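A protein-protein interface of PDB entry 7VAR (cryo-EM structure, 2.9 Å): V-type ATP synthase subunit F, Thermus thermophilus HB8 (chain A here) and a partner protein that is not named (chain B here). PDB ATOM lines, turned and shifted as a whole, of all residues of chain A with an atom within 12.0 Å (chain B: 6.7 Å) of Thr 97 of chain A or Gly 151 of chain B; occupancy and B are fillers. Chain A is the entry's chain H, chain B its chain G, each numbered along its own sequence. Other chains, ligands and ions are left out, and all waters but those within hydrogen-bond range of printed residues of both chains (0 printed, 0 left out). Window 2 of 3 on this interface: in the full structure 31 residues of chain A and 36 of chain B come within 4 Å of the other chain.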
ATOM      1  N   ASP A  54       8.521 -14.366  -0.528  1.00  0.00           N
ATOM      2  CA  ASP A  54       9.354 -14.895  -1.604  1.00  0.00           C
ATOM      3  C   ASP A  54      10.799 -14.480  -1.369  1.00  0.00           C
ATOM      4  O   ASP A  54      11.169 -13.317  -1.574  1.00  0.00           O
ATOM      5  CB  ASP A  54       8.868 -14.417  -2.974  1.00  0.00           C
ATOM      6  CG  ASP A  54       7.637 -15.162  -3.447  1.00  0.00           C
ATOM      7  OD1 ASP A  54       7.754 -16.364  -3.764  1.00  0.00           O
ATOM      8  OD2 ASP A  54       6.552 -14.546  -3.503  1.00  0.00           O
ATOM      9  N   MET A  63      21.052 -13.931  -8.614  1.00  0.00           N
ATOM     10  CA  MET A  63      20.675 -15.200  -9.234  1.00  0.00           C
ATOM     11  C   MET A  63      21.408 -15.442 -10.548  1.00  0.00           C
ATOM     12  O   MET A  63      21.724 -16.592 -10.877  1.00  0.00           O
ATOM     13  CB  MET A  63      19.166 -15.249  -9.470  1.00  0.00           C
ATOM     14  CG  MET A  63      18.685 -16.590 -10.006  1.00  0.00           C
ATOM     15  SD  MET A  63      16.936 -16.623 -10.429  1.00  0.00           S
ATOM     16  CE  MET A  63      16.790 -18.282 -11.090  1.00  0.00           C
ATOM     17  N   GLY A  88      -2.808 -23.820  -1.884  1.00  0.00           N
ATOM     18  CA  GLY A  88      -2.944 -22.528  -2.538  1.00  0.00           C
ATOM     19  C   GLY A  88      -1.642 -22.048  -3.147  1.00  0.00           C
ATOM     20  O   GLY A  88      -1.629 -21.470  -4.238  1.00  0.00           O
ATOM     21  N   TYR A  89      -0.527 -22.282  -2.452  1.00  0.00           N
ATOM     22  CA  TYR A  89       0.779 -21.920  -2.991  1.00  0.00           C
ATOM     23  C   TYR A  89       1.089 -22.720  -4.252  1.00  0.00           C
ATOM     24  O   TYR A  89       1.619 -22.178  -5.230  1.00  0.00           O
ATOM     25  CB  TYR A  89       1.844 -22.128  -1.913  1.00  0.00           C
ATOM     26  CG  TYR A  89       3.247 -22.385  -2.410  1.00  0.00           C
ATOM     27  CD1 TYR A  89       3.951 -21.408  -3.103  1.00  0.00           C
ATOM     28  CD2 TYR A  89       3.880 -23.596  -2.162  1.00  0.00           C
ATOM     29  CE1 TYR A  89       5.239 -21.636  -3.548  1.00  0.00           C
ATOM     30  CE2 TYR A  89       5.167 -23.833  -2.603  1.00  0.00           C
ATOM     31  CZ  TYR A  89       5.843 -22.850  -3.294  1.00  0.00           C
ATOM     32  OH  TYR A  89       7.124 -23.083  -3.738  1.00  0.00           O
ATOM     33  N   MET A  90       0.744 -24.011  -4.257  1.00  0.00           N
ATOM     34  CA  MET A  90       0.933 -24.827  -5.453  1.00  0.00           C
ATOM     35  C   MET A  90       0.042 -24.352  -6.597  1.00  0.00           C
ATOM     36  O   MET A  90       0.462 -24.351  -7.760  1.00  0.00           O
ATOM     37  CB  MET A  90       0.662 -26.296  -5.135  1.00  0.00           C
ATOM     38  CG  MET A  90       1.826 -26.996  -4.458  1.00  0.00           C
ATOM     39  SD  MET A  90       3.233 -27.211  -5.565  1.00  0.00           S
ATOM     40  CE  MET A  90       4.570 -27.351  -4.382  1.00  0.00           C
ATOM     41  N   ARG A  91      -1.197 -23.963  -6.288  1.00  0.00           N
ATOM     42  CA  ARG A  91      -2.081 -23.431  -7.319  1.00  0.00           C
ATOM     43  C   ARG A  91      -1.522 -22.143  -7.904  1.00  0.00           C
ATOM     44  O   ARG A  91      -1.602 -21.916  -9.116  1.00  0.00           O
ATOM     45  CB  ARG A  91      -3.481 -23.200  -6.750  1.00  0.00           C
ATOM     46  CG  ARG A  91      -4.274 -24.470  -6.449  1.00  0.00           C
ATOM     47  CD  ARG A  91      -4.479 -25.339  -7.688  1.00  0.00           C
ATOM     48  NE  ARG A  91      -3.372 -26.258  -7.927  1.00  0.00           N
ATOM     49  CZ  ARG A  91      -3.140 -27.355  -7.219  1.00  0.00           C
ATOM     50  NH1 ARG A  91      -3.928 -27.714  -6.218  1.00  0.00           N
ATOM     51  NH2 ARG A  91      -2.091 -28.115  -7.524  1.00  0.00           N
ATOM     52  N   GLU A  92      -0.951 -21.288  -7.056  1.00  0.00           N
ATOM     53  CA  GLU A  92      -0.288 -20.087  -7.553  1.00  0.00           C
ATOM     54  C   GLU A  92       0.900 -20.443  -8.440  1.00  0.00           C
ATOM     55  O   GLU A  92       1.123 -19.803  -9.474  1.00  0.00           O
ATOM     56  CB  GLU A  92       0.156 -19.207  -6.387  1.00  0.00           C
ATOM     57  CG  GLU A  92       0.351 -17.748  -6.760  1.00  0.00           C
ATOM     58  CD  GLU A  92      -0.900 -17.128  -7.349  1.00  0.00           C
ATOM     59  OE1 GLU A  92      -1.987 -17.305  -6.760  1.00  0.00           O
ATOM     60  OE2 GLU A  92      -0.798 -16.466  -8.403  1.00  0.00           O
ATOM     61  N   LEU A  93       1.670 -21.462  -8.052  1.00  0.00           N
ATOM     62  CA  LEU A  93       2.798 -21.896  -8.871  1.00  0.00           C
ATOM     63  C   LEU A  93       2.333 -22.351 -10.249  1.00  0.00           C
ATOM     64  O   LEU A  93       2.926 -21.988 -11.271  1.00  0.00           O
ATOM     65  CB  LEU A  93       3.553 -23.026  -8.173  1.00  0.00           C
ATOM     66  CG  LEU A  93       4.427 -22.689  -6.968  1.00  0.00           C
ATOM     67  CD1 LEU A  93       4.887 -23.975  -6.304  1.00  0.00           C
ATOM     68  CD2 LEU A  93       5.614 -21.834  -7.379  1.00  0.00           C
ATOM     69  N   VAL A  94       1.272 -23.157 -10.291  1.00  0.00           N
ATOM     70  CA  VAL A  94       0.754 -23.640 -11.568  1.00  0.00           C
ATOM     71  C   VAL A  94       0.212 -22.484 -12.400  1.00  0.00           C
ATOM     72  O   VAL A  94       0.417 -22.428 -13.618  1.00  0.00           O
ATOM     73  CB  VAL A  94      -0.312 -24.727 -11.342  1.00  0.00           C
ATOM     74  CG1 VAL A  94      -0.809 -25.262 -12.675  1.00  0.00           C
ATOM     75  CG2 VAL A  94       0.257 -25.857 -10.506  1.00  0.00           C
ATOM     76  N   ARG A  95      -0.498 -21.550 -11.761  1.00  0.00           N
ATOM     77  CA  ARG A  95      -1.049 -20.411 -12.487  1.00  0.00           C
ATOM     78  C   ARG A  95       0.060 -19.527 -13.044  1.00  0.00           C
ATOM     79  O   ARG A  95      -0.101 -18.905 -14.099  1.00  0.00           O
ATOM     80  CB  ARG A  95      -1.983 -19.618 -11.568  1.00  0.00           C
ATOM     81  CG  ARG A  95      -3.007 -18.734 -12.277  1.00  0.00           C
ATOM     82  CD  ARG A  95      -2.440 -17.369 -12.634  1.00  0.00           C
ATOM     83  NE  ARG A  95      -1.756 -16.760 -11.501  1.00  0.00           N
ATOM     84  CZ  ARG A  95      -0.782 -15.866 -11.606  1.00  0.00           C
ATOM     85  NH1 ARG A  95      -0.351 -15.449 -12.785  1.00  0.00           N
ATOM     86  NH2 ARG A  95      -0.226 -15.380 -10.501  1.00  0.00           N
ATOM     87  N   LYS A  96       1.195 -19.455 -12.348  1.00  0.00           N
ATOM     88  CA  LYS A  96       2.329 -18.705 -12.880  1.00  0.00           C
ATOM     89  C   LYS A  96       2.991 -19.455 -14.032  1.00  0.00           C
ATOM     90  O   LYS A  96       3.367 -18.852 -15.044  1.00  0.00           O
ATOM     91  CB  LYS A  96       3.339 -18.422 -11.767  1.00  0.00           C
ATOM     92  CG  LYS A  96       2.900 -17.341 -10.795  1.00  0.00           C
ATOM     93  CD  LYS A  96       3.900 -17.173  -9.666  1.00  0.00           C
ATOM     94  CE  LYS A  96       4.001 -18.434  -8.826  1.00  0.00           C
ATOM     95  NZ  LYS A  96       4.893 -18.254  -7.649  1.00  0.00           N
ATOM     96  N   THR A  97       3.135 -20.774 -13.895  1.00  0.00           N
ATOM     97  CA  THR A  97       3.843 -21.556 -14.905  1.00  0.00           C
ATOM     98  C   THR A  97       3.061 -21.626 -16.212  1.00  0.00           C
ATOM     99  O   THR A  97       3.617 -21.400 -17.292  1.00  0.00           O
ATOM    100  CB  THR A  97       4.124 -22.962 -14.374  1.00  0.00           C
ATOM    101  OG1 THR A  97       4.963 -22.878 -13.215  1.00  0.00           O
ATOM    102  CG2 THR A  97       4.813 -23.802 -15.436  1.00  0.00           C
ATOM    103  N   ILE A  98       1.769 -21.943 -16.137  1.00  0.00           N
ATOM    104  CA  ILE A  98       0.969 -22.145 -17.339  1.00  0.00           C
ATOM    105  C   ILE A  98       0.092 -20.941 -17.678  1.00  0.00           C
ATOM    106  O   ILE A  98      -0.114 -20.657 -18.869  1.00  0.00           O
ATOM    107  CB  ILE A  98       0.108 -23.420 -17.205  1.00  0.00           C
ATOM    108  CG1 ILE A  98       1.008 -24.647 -17.044  1.00  0.00           C
ATOM    109  CG2 ILE A  98      -0.801 -23.601 -18.411  1.00  0.00           C
ATOM    110  CD1 ILE A  98       0.250 -25.943 -16.880  1.00  0.00           C
ATOM    111  N   GLY A  99      -0.397 -20.207 -16.681  1.00  0.00           N
ATOM    112  CA  GLY A  99      -1.236 -19.052 -16.918  1.00  0.00           C
ATOM    113  C   GLY A  99      -2.708 -19.249 -16.632  1.00  0.00           C
ATOM    114  O   GLY A  99      -3.498 -18.339 -16.910  1.00  0.00           O
ATOM    115  N   PHE A 100      -3.105 -20.399 -16.092  1.00  0.00           N
ATOM    116  CA  PHE A 100      -4.511 -20.682 -15.844  1.00  0.00           C
ATOM    117  C   PHE A 100      -4.642 -21.563 -14.612  1.00  0.00           C
ATOM    118  O   PHE A 100      -3.724 -22.310 -14.264  1.00  0.00           O
ATOM    119  CB  PHE A 100      -5.165 -21.369 -17.049  1.00  0.00           C
ATOM    120  CG  PHE A 100      -5.012 -20.612 -18.338  1.00  0.00           C
ATOM    121  CD1 PHE A 100      -5.873 -19.575 -18.654  1.00  0.00           C
ATOM    122  CD2 PHE A 100      -3.999 -20.933 -19.228  1.00  0.00           C
ATOM    123  CE1 PHE A 100      -5.731 -18.875 -19.837  1.00  0.00           C
ATOM    124  CE2 PHE A 100      -3.852 -20.234 -20.411  1.00  0.00           C
ATOM    125  CZ  PHE A 100      -4.719 -19.205 -20.717  1.00  0.00           C
ATOM    126  N   ASP A 101      -5.794 -21.463 -13.952  1.00  0.00           N
ATOM    127  CA  ASP A 101      -6.109 -22.375 -12.862  1.00  0.00           C
ATOM    128  C   ASP A 101      -6.372 -23.772 -13.413  1.00  0.00           C
ATOM    129  O   ASP A 101      -6.953 -23.943 -14.488  1.00  0.00           O
ATOM    130  CB  ASP A 101      -7.320 -21.873 -12.075  1.00  0.00           C
ATOM    131  CG  ASP A 101      -8.471 -21.468 -12.972  1.00  0.00           C
ATOM    132  OD1 ASP A 101      -8.223 -21.162 -14.158  1.00  0.00           O
ATOM    133  OD2 ASP A 101      -9.622 -21.446 -12.489  1.00  0.00           O
ATOM    134  N   ILE A 102      -5.937 -24.784 -12.659  1.00  0.00           N
ATOM    135  CA  ILE A 102      -5.854 -26.145 -13.172  1.00  0.00           C
ATOM    136  C   ILE A 102      -6.690 -27.139 -12.380  1.00  0.00           C
ATOM    137  O   ILE A 102      -6.821 -28.289 -12.801  1.00  0.00           O
ATOM    138  CB  ILE A 102      -4.386 -26.616 -13.236  1.00  0.00           C
ATOM    139  CG1 ILE A 102      -4.197 -27.662 -14.334  1.00  0.00           C
ATOM    140  CG2 ILE A 102      -3.932 -27.156 -11.886  1.00  0.00           C
ATOM    141  CD1 ILE A 102      -4.302 -27.094 -15.728  1.00  0.00           C
ATOM    142  N   PHE B  39       5.162 -32.279 -16.036  1.00  0.00           N
ATOM    143  CA  PHE B  39       4.996 -31.221 -15.045  1.00  0.00           C
ATOM    144  C   PHE B  39       3.892 -31.554 -14.053  1.00  0.00           C
ATOM    145  O   PHE B  39       4.001 -31.233 -12.864  1.00  0.00           O
ATOM    146  CB  PHE B  39       4.700 -29.900 -15.753  1.00  0.00           C
ATOM    147  CG  PHE B  39       4.511 -28.737 -14.824  1.00  0.00           C
ATOM    148  CD1 PHE B  39       5.600 -28.098 -14.261  1.00  0.00           C
ATOM    149  CD2 PHE B  39       3.241 -28.276 -14.525  1.00  0.00           C
ATOM    150  CE1 PHE B  39       5.425 -27.024 -13.412  1.00  0.00           C
ATOM    151  CE2 PHE B  39       3.060 -27.204 -13.677  1.00  0.00           C
ATOM    152  CZ  PHE B  39       4.154 -26.577 -13.119  1.00  0.00           C
ATOM    153  N   ARG B 146      13.288 -29.148  -9.439  1.00  0.00           N
ATOM    154  CA  ARG B 146      12.941 -29.851 -10.672  1.00  0.00           C
ATOM    155  C   ARG B 146      11.681 -29.265 -11.301  1.00  0.00           C
ATOM    156  O   ARG B 146      11.614 -29.084 -12.527  1.00  0.00           O
ATOM    157  CB  ARG B 146      12.771 -31.346 -10.403  1.00  0.00           C
ATOM    158  CG  ARG B 146      14.091 -32.076 -10.203  1.00  0.00           C
ATOM    159  CD  ARG B 146      13.958 -33.583 -10.381  1.00  0.00           C
ATOM    160  NE  ARG B 146      13.851 -33.963 -11.785  1.00  0.00           N
ATOM    161  CZ  ARG B 146      12.780 -34.519 -12.333  1.00  0.00           C
ATOM    162  NH1 ARG B 146      11.709 -34.810 -11.616  1.00  0.00           N
ATOM    163  NH2 ARG B 146      12.787 -34.799 -13.633  1.00  0.00           N
ATOM    164  N   LEU B 147      10.678 -28.947 -10.478  1.00  0.00           N
ATOM    165  CA  LEU B 147       9.450 -28.356 -11.001  1.00  0.00           C
ATOM    166  C   LEU B 147       9.724 -27.004 -11.652  1.00  0.00           C
ATOM    167  O   LEU B 147       9.174 -26.692 -12.716  1.00  0.00           O
ATOM    168  CB  LEU B 147       8.423 -28.220  -9.875  1.00  0.00           C
ATOM    169  CG  LEU B 147       6.994 -27.823 -10.246  1.00  0.00           C
ATOM    170  CD1 LEU B 147       6.012 -28.559  -9.357  1.00  0.00           C
ATOM    171  CD2 LEU B 147       6.793 -26.322 -10.120  1.00  0.00           C
ATOM    172  N   LYS B 148      10.568 -26.185 -11.022  1.00  0.00           N
ATOM    173  CA  LYS B 148      10.890 -24.879 -11.590  1.00  0.00           C
ATOM    174  C   LYS B 148      11.605 -25.019 -12.928  1.00  0.00           C
ATOM    175  O   LYS B 148      11.329 -24.266 -13.870  1.00  0.00           O
ATOM    176  CB  LYS B 148      11.742 -24.072 -10.611  1.00  0.00           C
ATOM    177  CG  LYS B 148      11.014 -23.666  -9.342  1.00  0.00           C
ATOM    178  CD  LYS B 148       9.953 -22.619  -9.626  1.00  0.00           C
ATOM    179  CE  LYS B 148       9.125 -22.331  -8.385  1.00  0.00           C
ATOM    180  NZ  LYS B 148       9.912 -21.611  -7.347  1.00  0.00           N
ATOM    181  N   LYS B 149      12.535 -25.972 -13.029  1.00  0.00           N
ATOM    182  CA  LYS B 149      13.224 -26.173 -14.301  1.00  0.00           C
ATOM    183  C   LYS B 149      12.258 -26.627 -15.390  1.00  0.00           C
ATOM    184  O   LYS B 149      12.335 -26.158 -16.537  1.00  0.00           O
ATOM    185  CB  LYS B 149      14.362 -27.176 -14.131  1.00  0.00           C
ATOM    186  CG  LYS B 149      15.701 -26.526 -13.828  1.00  0.00           C
ATOM    187  CD  LYS B 149      16.239 -25.792 -15.046  1.00  0.00           C
ATOM    188  CE  LYS B 149      17.439 -24.930 -14.691  1.00  0.00           C
ATOM    189  NZ  LYS B 149      17.805 -24.006 -15.799  1.00  0.00           N
ATOM    190  N   ILE B 150      11.336 -27.532 -15.052  1.00  0.00           N
ATOM    191  CA  ILE B 150      10.352 -27.983 -16.034  1.00  0.00           C
ATOM    192  C   ILE B 150       9.475 -26.820 -16.484  1.00  0.00           C
ATOM    193  O   ILE B 150       9.157 -26.683 -17.673  1.00  0.00           O
ATOM    194  CB  ILE B 150       9.516 -29.142 -15.464  1.00  0.00           C
ATOM    195  CG1 ILE B 150      10.404 -30.358 -15.203  1.00  0.00           C
ATOM    196  CG2 ILE B 150       8.383 -29.504 -16.412  1.00  0.00           C
ATOM    197  CD1 ILE B 150      10.832 -31.084 -16.458  1.00  0.00           C
ATOM    198  N   GLY B 151       9.068 -25.966 -15.543  1.00  0.00           N
ATOM    199  CA  GLY B 151       8.272 -24.805 -15.909  1.00  0.00           C
ATOM    200  C   GLY B 151       9.020 -23.839 -16.807  1.00  0.00           C
ATOM    201  O   GLY B 151       8.445 -23.270 -17.741  1.00  0.00           O
ATOM    202  N   GLU B 152      10.310 -23.632 -16.532  1.00  0.00           N
ATOM    203  CA  GLU B 152      11.125 -22.789 -17.400  1.00  0.00           C
ATOM    204  C   GLU B 152      11.182 -23.353 -18.814  1.00  0.00           C
ATOM    205  O   GLU B 152      11.054 -22.610 -19.797  1.00  0.00           O
ATOM    206  CB  GLU B 152      12.536 -22.652 -16.828  1.00  0.00           C
ATOM    207  CG  GLU B 152      12.639 -21.737 -15.619  1.00  0.00           C
ATOM    208  CD  GLU B 152      14.076 -21.386 -15.278  1.00  0.00           C
ATOM    209  OE1 GLU B 152      14.989 -22.113 -15.722  1.00  0.00           O
ATOM    210  OE2 GLU B 152      14.292 -20.384 -14.566  1.00  0.00           O
ATOM    211  N   GLU B 153      11.372 -24.670 -18.933  1.00  0.00           N
ATOM    212  CA  GLU B 153      11.396 -25.288 -20.257  1.00  0.00           C
ATOM    213  C   GLU B 153      10.057 -25.134 -20.971  1.00  0.00           C
ATOM    214  O   GLU B 153      10.019 -24.873 -22.180  1.00  0.00           O
ATOM    215  CB  GLU B 153      11.779 -26.763 -20.142  1.00  0.00           C
ATOM    216  CG  GLU B 153      13.222 -26.996 -19.728  1.00  0.00           C
ATOM    217  CD  GLU B 153      14.214 -26.484 -20.756  1.00  0.00           C
ATOM    218  OE1 GLU B 153      13.862 -26.436 -21.954  1.00  0.00           O
ATOM    219  OE2 GLU B 153      15.346 -26.128 -20.366  1.00  0.00           O
ATOM    220  N   ILE B 154       8.950 -25.294 -20.242  1.00  0.00           N
ATOM    221  CA  ILE B 154       7.629 -25.136 -20.851  1.00  0.00           C
ATOM    222  C   ILE B 154       7.443 -23.714 -21.363  1.00  0.00           C
ATOM    223  O   ILE B 154       6.948 -23.495 -22.477  1.00  0.00           O
ATOM    224  CB  ILE B 154       6.527 -25.523 -19.849  1.00  0.00           C
ATOM    225  CG1 ILE B 154       6.475 -27.039 -19.666  1.00  0.00           C
ATOM    226  CG2 ILE B 154       5.177 -24.997 -20.309  1.00  0.00           C
ATOM    227  CD1 ILE B 154       5.528 -27.486 -18.578  1.00  0.00           C
ATOM    228  N   LYS B 155       7.833 -22.725 -20.555  1.00  0.00           N
ATOM    229  CA  LYS B 155       7.731 -21.330 -20.972  1.00  0.00           C
ATOM    230  C   LYS B 155       8.555 -21.074 -22.228  1.00  0.00           C
ATOM    231  O   LYS B 155       8.096 -20.414 -23.170  1.00  0.00           O
ATOM    232  CB  LYS B 155       8.187 -20.413 -19.837  1.00  0.00           C
ATOM    233  CG  LYS B 155       7.175 -20.233 -18.720  1.00  0.00           C
ATOM    234  CD  LYS B 155       6.125 -19.202 -19.099  1.00  0.00           C
ATOM    235  CE  LYS B 155       5.327 -18.755 -17.886  1.00  0.00           C
ATOM    236  NZ  LYS B 155       4.428 -17.611 -18.206  1.00  0.00           N
ATOM    237  N   LYS B 156       9.785 -21.589 -22.252  1.00  0.00           N
ATOM    238  CA  LYS B 156      10.658 -21.383 -23.403  1.00  0.00           C
ATOM    239  C   LYS B 156      10.061 -22.003 -24.663  1.00  0.00           C
ATOM    240  O   LYS B 156      10.079 -21.392 -25.739  1.00  0.00           O
ATOM    241  CB  LYS B 156      12.039 -21.966 -23.112  1.00  0.00           C
ATOM    242  CG  LYS B 156      13.115 -21.563 -24.100  1.00  0.00           C
ATOM    243  CD  LYS B 156      14.492 -21.923 -23.570  1.00  0.00           C
ATOM    244  CE  LYS B 156      15.580 -21.575 -24.570  1.00  0.00           C
ATOM    245  NZ  LYS B 156      15.625 -22.556 -25.688  1.00  0.00           N
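Of the 17 printed residues of chain A, 3 touch a printed residue of chain B.
Hydrophobic or aromatic side chains of chain A that line the printed part of chain B: Leu 93.
Along chain A the printed residues that touch a printed residue of chain B span positions 93 to 97.
Of the 12 printed residues of chain B, 4 touch a printed residue of chain A.
Printed residues of chain B that touch a printed residue of chain A: Phe 39, Lys 148, Gly 151 and Lys 155.
Among the printed residues, 5 pairs touch across the chains.
Among the printed residues, no Asp or Glu carboxylate lies within 4 Å of a Lys or Arg side-chain nitrogen of the other chain.
The backbone carbonyl oxygen of Leu 93 of chain A lies within hydrogen-bond range of the side-chain hydroxyl of Thr 97 of chain A (3.0 Å).
Among the printed residues, pairs that only touch across the chains: Thr 97 of chain A with Lys 155 of chain B (3.2 Å), Lys 96 of chain A with Lys 155 of chain B (3.5 Å), Thr 97 of chain A with Gly 151 of chain B (3.6 Å), Thr 97 of chain A with Phe 39 of chain B (3.7 Å) and Leu 93 of chain A with Lys 148 of chain B (3.7 Å).
Glu 92 of chain A touches none of the printed residues of chain B.
Printed residues of chain B within 4 Å of Leu 93 of chain A: Lys 148 (3.7 Å).
Printed residues of chain B within 4 Å of Lys 96 of chain A: Lys 155.
Printed residues of chain B within 4 Å of Thr 97 of chain A: Phe 39 (3.7 Å), Gly 151 (3.6 Å) and Lys 155 (3.2 Å).
Asp 101 of chain A touches none of the printed residues of chain B.
Phe 39 of chain B touches one residue of chain A.
Leu 147 of chain B touches none of the printed residues of chain A.
Of chain A, only Leu 93 comes within 4 Å of Lys 148 of chain B.
No residue of chain A comes within 4 Å of Ile 150 of chain B.
Of chain A, only Thr 97 (3.6 Å) comes within 4 Å of Gly 151 of chain B.
Glu 152 of chain B touches none of the printed residues of chain A.
Glu 153 of chain B touches none of the printed residues of chain A.
Lys 155 of chain B touches just these residues of chain A: Lys 96 (3.5 Å) and Thr 97 (3.2 Å).
The nearest residue of chain B that does not touch Thr 97 of chain A is Ile 154 of chain B (4.9 Å).
The nearest residue of chain A that does not touch Gly 151 of chain B is Ile 98 of chain A (7.0 Å).
The nearest printed residue of chain B that does not touch Leu 93 of chain A is Leu 147 of chain B (4.9 Å).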
